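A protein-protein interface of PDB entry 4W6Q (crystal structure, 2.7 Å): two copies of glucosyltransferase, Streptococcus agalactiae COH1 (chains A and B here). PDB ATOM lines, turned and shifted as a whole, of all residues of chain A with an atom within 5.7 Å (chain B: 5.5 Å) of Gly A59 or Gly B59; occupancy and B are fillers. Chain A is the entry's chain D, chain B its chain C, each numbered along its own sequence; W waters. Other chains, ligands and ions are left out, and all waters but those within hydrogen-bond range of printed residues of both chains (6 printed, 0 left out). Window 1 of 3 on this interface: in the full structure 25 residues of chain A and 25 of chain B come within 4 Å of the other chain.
Printed residues of chain B within 4 Å of Lys A55: Arg B56.
Printed residues of chain B within 4 Å of Asp A58: Arg B56 (3.1 Å).
Of chain B, only Arg B56, Gly B59 and Ile B60 come within 4 Å of Gly A59.
Gly B59 touches just these residues of chain A: Arg A56, Gly A59 and Ile A60.
Of the printed residues of chain A, Ile B60 touches Gly A59.
The backbone carbonyl oxygen (O) of Gly A59 sits at hydrogen-bond distance from the side-chain hydroxyl (OG) of Ser A62, at 3.5 Å.
OG of Ser B62 lies within hydrogen-bond range of O of Gly B59 (3.5 Å).
Printed residues of chain B that touch a printed residue of chain A: Gly B39, Lys B55, Arg B56, Asp B58, Gly B59, Ile B60 and Ser B62.
Of the 10 printed residues of chain A, 7 touch a printed residue of chain B.
NH2 of Arg A56 is in salt-bridge range of OD2 of Asp B58 (3.997 Å).
NH2 of Arg B56 lies within salt-bridge range of OD2 of Asp A58 (3.8 Å).
The backbone NH of Ile B60 lies close to the backbone carbonyl oxygen of Gly A59 (3.4 Å).
O of Gly B39 lies within hydrogen-bond range of OG of Ser A62 (2.8 Å).
OG of Ser B62 is in hydrogen-bond range of O of Gly A39 (2.9 Å).
Gly A39 touches Ser B62, and with the chains exchanged Ser A62 touches Gly B39.
Lys A55 touches Arg B56, and with the chains exchanged Arg A56 touches Lys B55.
Arg B56 touches its own counterpart, Arg A56.
Gly A59 touches Ile B60, and with the chains exchanged Ile A60 touches Gly B59.
10 positions are printed for both chains.
Of the 12 pairs that touch across the chains among the printed residues, 12 have their exchanged pair printed and touching as well.
Water W1 bridges the side-chain carboxylate (OD2) of Asp B58 and the guanidinium group (NH2) of Arg A56.
Water W3 lies within hydrogen-bond range of the backbone carbonyl oxygen (O) of Gly B59, the backbone carbonyl oxygen (O) of Gly A39 and the side-chain hydroxyl (OG) of Ser B62.
Water W5 bridges OD2 of Asp A58 and NH2 of Arg B56.
Water W2 lies within hydrogen-bond range of O of Gly A59 (2.8 Å), O of Gly B39 (2.8 Å) and OG of Ser A62 (3.0 Å).
Water W4 lies within hydrogen-bond range of the backbone carbonyl oxygen (O) of Asp A58 (2.8 Å), the backbone NH (N) of Gly A59 (3.3 Å) and the guanidinium group (NH2) of Arg B56 (3.3 Å).
Water W6 lies within hydrogen-bond range of O of Asp B58 (2.9 Å) and NE of Arg A56 (3.2 Å).
Lys A55 touches Arg B56.
O of Lys B55 touches CB of Arg A56 (3.1 Å).
CA of Arg A56 touches CA of Arg B56 (3.7 Å).
O of Arg A56 touches CA of Gly B59, at 3.8 Å.
Arg B56 touches Gly A59 (O to CA, 3.8 Å).
Gly A59 touches Gly B59.
Gly B59 touches Ile A60.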
ATOM      1  N   GLY A  39      -2.948  -2.457  -8.327  1.00  0.00           N
ATOM      2  CA  GLY A  39      -1.686  -2.310  -9.032  1.00  0.00           C
ATOM      3  C   GLY A  39      -1.660  -1.103  -9.952  1.00  0.00           C
ATOM      4  O   GLY A  39      -2.679  -0.750 -10.539  1.00  0.00           O
ATOM      5  N   SER A  54      -8.760   7.211 -19.106  1.00  0.00           N
ATOM      6  CA  SER A  54      -9.855   7.030 -18.169  1.00  0.00           C
ATOM      7  C   SER A  54     -10.260   5.571 -18.047  1.00  0.00           C
ATOM      8  O   SER A  54     -10.738   5.125 -16.999  1.00  0.00           O
ATOM      9  CB  SER A  54     -11.058   7.864 -18.608  1.00  0.00           C
ATOM     10  OG  SER A  54     -12.173   7.632 -17.769  1.00  0.00           O
ATOM     11  N   LYS A  55     -10.072   4.828 -19.126  1.00  0.00           N
ATOM     12  CA  LYS A  55     -10.549   3.462 -19.171  1.00  0.00           C
ATOM     13  C   LYS A  55      -9.500   2.543 -18.588  1.00  0.00           C
ATOM     14  O   LYS A  55      -9.827   1.504 -18.025  1.00  0.00           O
ATOM     15  CB  LYS A  55     -10.912   3.055 -20.605  1.00  0.00           C
ATOM     16  CG  LYS A  55     -12.030   3.901 -21.208  1.00  0.00           C
ATOM     17  CD  LYS A  55     -12.844   3.162 -22.258  1.00  0.00           C
ATOM     18  CE  LYS A  55     -13.917   4.091 -22.841  1.00  0.00           C
ATOM     19  NZ  LYS A  55     -14.900   3.408 -23.734  1.00  0.00           N
ATOM     20  N   ARG A  56      -8.237   2.935 -18.726  1.00  0.00           N
ATOM     21  CA  ARG A  56      -7.145   2.215 -18.090  1.00  0.00           C
ATOM     22  C   ARG A  56      -7.334   2.283 -16.588  1.00  0.00           C
ATOM     23  O   ARG A  56      -7.282   1.265 -15.900  1.00  0.00           O
ATOM     24  CB  ARG A  56      -5.797   2.799 -18.486  1.00  0.00           C
ATOM     25  CG  ARG A  56      -4.681   2.448 -17.545  1.00  0.00           C
ATOM     26  CD  ARG A  56      -3.413   3.239 -17.847  1.00  0.00           C
ATOM     27  NE  ARG A  56      -2.438   2.423 -18.551  1.00  0.00           N
ATOM     28  CZ  ARG A  56      -2.066   2.632 -19.806  1.00  0.00           C
ATOM     29  NH1 ARG A  56      -2.585   3.646 -20.476  1.00  0.00           N
ATOM     30  NH2 ARG A  56      -1.180   1.830 -20.384  1.00  0.00           N
ATOM     31  N   LEU A  57      -7.573   3.491 -16.094  1.00  0.00           N
ATOM     32  CA  LEU A  57      -7.899   3.694 -14.693  1.00  0.00           C
ATOM     33  C   LEU A  57      -9.099   2.864 -14.285  1.00  0.00           C
ATOM     34  O   LEU A  57      -9.119   2.272 -13.211  1.00  0.00           O
ATOM     35  CB  LEU A  57      -8.184   5.162 -14.411  1.00  0.00           C
ATOM     36  CG  LEU A  57      -6.990   6.062 -14.134  1.00  0.00           C
ATOM     37  CD1 LEU A  57      -7.485   7.391 -13.600  1.00  0.00           C
ATOM     38  CD2 LEU A  57      -6.049   5.394 -13.162  1.00  0.00           C
ATOM     39  N   ASP A  58     -10.101   2.828 -15.152  1.00  0.00           N
ATOM     40  CA  ASP A  58     -11.321   2.093 -14.867  1.00  0.00           C
ATOM     41  C   ASP A  58     -11.006   0.623 -14.634  1.00  0.00           C
ATOM     42  O   ASP A  58     -11.678  -0.057 -13.854  1.00  0.00           O
ATOM     43  CB  ASP A  58     -12.327   2.259 -16.006  1.00  0.00           C
ATOM     44  CG  ASP A  58     -13.180   3.502 -15.850  1.00  0.00           C
ATOM     45  OD1 ASP A  58     -13.143   4.104 -14.753  1.00  0.00           O
ATOM     46  OD2 ASP A  58     -13.899   3.868 -16.808  1.00  0.00           O
ATOM     47  N   GLY A  59      -9.963   0.153 -15.305  1.00  0.00           N
ATOM     48  CA  GLY A  59      -9.520  -1.219 -15.185  1.00  0.00           C
ATOM     49  C   GLY A  59      -8.624  -1.415 -13.982  1.00  0.00           C
ATOM     50  O   GLY A  59      -8.448  -2.534 -13.508  1.00  0.00           O
ATOM     51  N   ILE A  60      -8.045  -0.324 -13.491  1.00  0.00           N
ATOM     52  CA  ILE A  60      -7.265  -0.383 -12.269  1.00  0.00           C
ATOM     53  C   ILE A  60      -8.217  -0.533 -11.080  1.00  0.00           C
ATOM     54  O   ILE A  60      -7.923  -1.250 -10.118  1.00  0.00           O
ATOM     55  CB  ILE A  60      -6.376   0.868 -12.097  1.00  0.00           C
ATOM     56  CG1 ILE A  60      -5.383   0.976 -13.244  1.00  0.00           C
ATOM     57  CG2 ILE A  60      -5.601   0.812 -10.787  1.00  0.00           C
ATOM     58  CD1 ILE A  60      -4.435   2.137 -13.103  1.00  0.00           C
ATOM     59  N   CYS A  61      -9.373   0.118 -11.193  1.00  0.00           N
ATOM     60  CA  CYS A  61     -10.357   0.228 -10.120  1.00  0.00           C
ATOM     61  C   CYS A  61     -11.534  -0.753 -10.182  1.00  0.00           C
ATOM     62  O   CYS A  61     -12.439  -0.692  -9.347  1.00  0.00           O
ATOM     63  CB  CYS A  61     -10.921   1.647 -10.107  1.00  0.00           C
ATOM     64  SG  CYS A  61      -9.983   2.768  -9.086  1.00  0.00           S
ATOM     65  N   SER A  62     -11.522  -1.653 -11.157  1.00  0.00           N
ATOM     66  CA  SER A  62     -12.673  -2.518 -11.404  1.00  0.00           C
ATOM     67  C   SER A  62     -13.042  -3.473 -10.267  1.00  0.00           C
ATOM     68  O   SER A  62     -14.097  -4.091 -10.308  1.00  0.00           O
ATOM     69  CB  SER A  62     -12.429  -3.333 -12.667  1.00  0.00           C
ATOM     70  OG  SER A  62     -11.324  -4.190 -12.491  1.00  0.00           O
ATOM     71  N   GLY B  39      -9.077  -7.534 -10.158  1.00  0.00           N
ATOM     72  CA  GLY B  39     -10.447  -7.092 -10.321  1.00  0.00           C
ATOM     73  C   GLY B  39     -10.845  -6.999 -11.777  1.00  0.00           C
ATOM     74  O   GLY B  39     -10.047  -6.633 -12.632  1.00  0.00           O
ATOM     75  N   SER B  54      -7.566  -2.378 -24.720  1.00  0.00           N
ATOM     76  CA  SER B  54      -6.281  -3.005 -24.504  1.00  0.00           C
ATOM     77  C   SER B  54      -5.586  -2.309 -23.337  1.00  0.00           C
ATOM     78  O   SER B  54      -4.876  -2.942 -22.563  1.00  0.00           O
ATOM     79  CB  SER B  54      -5.442  -2.935 -25.779  1.00  0.00           C
ATOM     80  OG  SER B  54      -4.595  -4.057 -25.895  1.00  0.00           O
ATOM     81  N   LYS B  55      -5.844  -1.013 -23.190  1.00  0.00           N
ATOM     82  CA  LYS B  55      -5.228  -0.206 -22.141  1.00  0.00           C
ATOM     83  C   LYS B  55      -5.944  -0.348 -20.792  1.00  0.00           C
ATOM     84  O   LYS B  55      -5.389  -0.039 -19.735  1.00  0.00           O
ATOM     85  CB  LYS B  55      -5.182   1.268 -22.564  1.00  0.00           C
ATOM     86  CG  LYS B  55      -4.061   1.591 -23.546  1.00  0.00           C
ATOM     87  CD  LYS B  55      -4.096   3.042 -23.994  1.00  0.00           C
ATOM     88  CE  LYS B  55      -2.989   3.345 -25.009  1.00  0.00           C
ATOM     89  NZ  LYS B  55      -1.644   3.434 -24.368  1.00  0.00           N
ATOM     90  N   ARG B  56      -7.182  -0.812 -20.827  1.00  0.00           N
ATOM     91  CA  ARG B  56      -7.875  -1.128 -19.598  1.00  0.00           C
ATOM     92  C   ARG B  56      -7.446  -2.535 -19.161  1.00  0.00           C
ATOM     93  O   ARG B  56      -7.452  -2.874 -17.972  1.00  0.00           O
ATOM     94  CB  ARG B  56      -9.391  -1.022 -19.789  1.00  0.00           C
ATOM     95  CG  ARG B  56     -10.091  -2.328 -20.102  1.00  0.00           C
ATOM     96  CD  ARG B  56     -11.592  -2.118 -20.194  1.00  0.00           C
ATOM     97  NE  ARG B  56     -12.057  -1.195 -19.168  1.00  0.00           N
ATOM     98  CZ  ARG B  56     -13.063  -0.351 -19.330  1.00  0.00           C
ATOM     99  NH1 ARG B  56     -13.707  -0.316 -20.482  1.00  0.00           N
ATOM    100  NH2 ARG B  56     -13.417   0.458 -18.344  1.00  0.00           N
ATOM    101  N   LEU B  57      -7.065  -3.351 -20.136  1.00  0.00           N
ATOM    102  CA  LEU B  57      -6.521  -4.654 -19.830  1.00  0.00           C
ATOM    103  C   LEU B  57      -5.192  -4.427 -19.138  1.00  0.00           C
ATOM    104  O   LEU B  57      -4.905  -5.041 -18.114  1.00  0.00           O
ATOM    105  CB  LEU B  57      -6.365  -5.487 -21.092  1.00  0.00           C
ATOM    106  CG  LEU B  57      -7.698  -6.091 -21.512  1.00  0.00           C
ATOM    107  CD1 LEU B  57      -7.587  -6.850 -22.818  1.00  0.00           C
ATOM    108  CD2 LEU B  57      -8.181  -7.009 -20.401  1.00  0.00           C
ATOM    109  N   ASP B  58      -4.418  -3.492 -19.688  1.00  0.00           N
ATOM    110  CA  ASP B  58      -3.155  -3.066 -19.103  1.00  0.00           C
ATOM    111  C   ASP B  58      -3.307  -2.511 -17.699  1.00  0.00           C
ATOM    112  O   ASP B  58      -2.336  -2.440 -16.962  1.00  0.00           O
ATOM    113  CB  ASP B  58      -2.486  -2.000 -19.973  1.00  0.00           C
ATOM    114  CG  ASP B  58      -1.990  -2.548 -21.283  1.00  0.00           C
ATOM    115  OD1 ASP B  58      -2.024  -3.784 -21.458  1.00  0.00           O
ATOM    116  OD2 ASP B  58      -1.549  -1.745 -22.132  1.00  0.00           O
ATOM    117  N   GLY B  59      -4.511  -2.082 -17.350  1.00  0.00           N
ATOM    118  CA  GLY B  59      -4.763  -1.538 -16.033  1.00  0.00           C
ATOM    119  C   GLY B  59      -5.184  -2.629 -15.065  1.00  0.00           C
ATOM    120  O   GLY B  59      -4.858  -2.595 -13.874  1.00  0.00           O
ATOM    121  N   ILE B  60      -5.917  -3.608 -15.579  1.00  0.00           N
ATOM    122  CA  ILE B  60      -6.305  -4.735 -14.755  1.00  0.00           C
ATOM    123  C   ILE B  60      -5.037  -5.507 -14.358  1.00  0.00           C
ATOM    124  O   ILE B  60      -4.966  -6.087 -13.287  1.00  0.00           O
ATOM    125  CB  ILE B  60      -7.337  -5.631 -15.496  1.00  0.00           C
ATOM    126  CG1 ILE B  60      -8.654  -4.869 -15.667  1.00  0.00           C
ATOM    127  CG2 ILE B  60      -7.613  -6.927 -14.748  1.00  0.00           C
ATOM    128  CD1 ILE B  60      -9.720  -5.627 -16.419  1.00  0.00           C
ATOM    129  N   CYS B  61      -4.014  -5.440 -15.199  1.00  0.00           N
ATOM    130  CA  CYS B  61      -2.878  -6.341 -15.095  1.00  0.00           C
ATOM    131  C   CYS B  61      -1.573  -5.689 -14.687  1.00  0.00           C
ATOM    132  O   CYS B  61      -0.539  -6.364 -14.617  1.00  0.00           O
ATOM    133  CB  CYS B  61      -2.659  -7.044 -16.430  1.00  0.00           C
ATOM    134  SG  CYS B  61      -3.931  -8.227 -16.815  1.00  0.00           S
ATOM    135  N   SER B  62      -1.609  -4.391 -14.424  1.00  0.00           N
ATOM    136  CA  SER B  62      -0.368  -3.656 -14.205  1.00  0.00           C
ATOM    137  C   SER B  62       0.508  -4.286 -13.111  1.00  0.00           C
ATOM    138  O   SER B  62       1.730  -4.330 -13.243  1.00  0.00           O
ATOM    139  CB  SER B  62      -0.675  -2.194 -13.876  1.00  0.00           C
ATOM    140  OG  SER B  62      -1.606  -2.093 -12.821  1.00  0.00           O
HETATM  141  O   HOH W   1       0.365  -0.506 -21.358  1.00  0.00           O
HETATM  142  O   HOH W   2      -8.542  -4.522 -11.563  1.00  0.00           O
HETATM  143  O   HOH W   3      -4.161  -2.882 -11.335  1.00  0.00           O
HETATM  144  O   HOH W   4     -12.627  -1.657 -15.929  1.00  0.00           O
HETATM  145  O   HOH W   5     -15.966   2.098 -17.326  1.00  0.00           O
HETATM  146  O   HOH W   6      -0.792  -0.062 -17.344  1.00  0.00           O
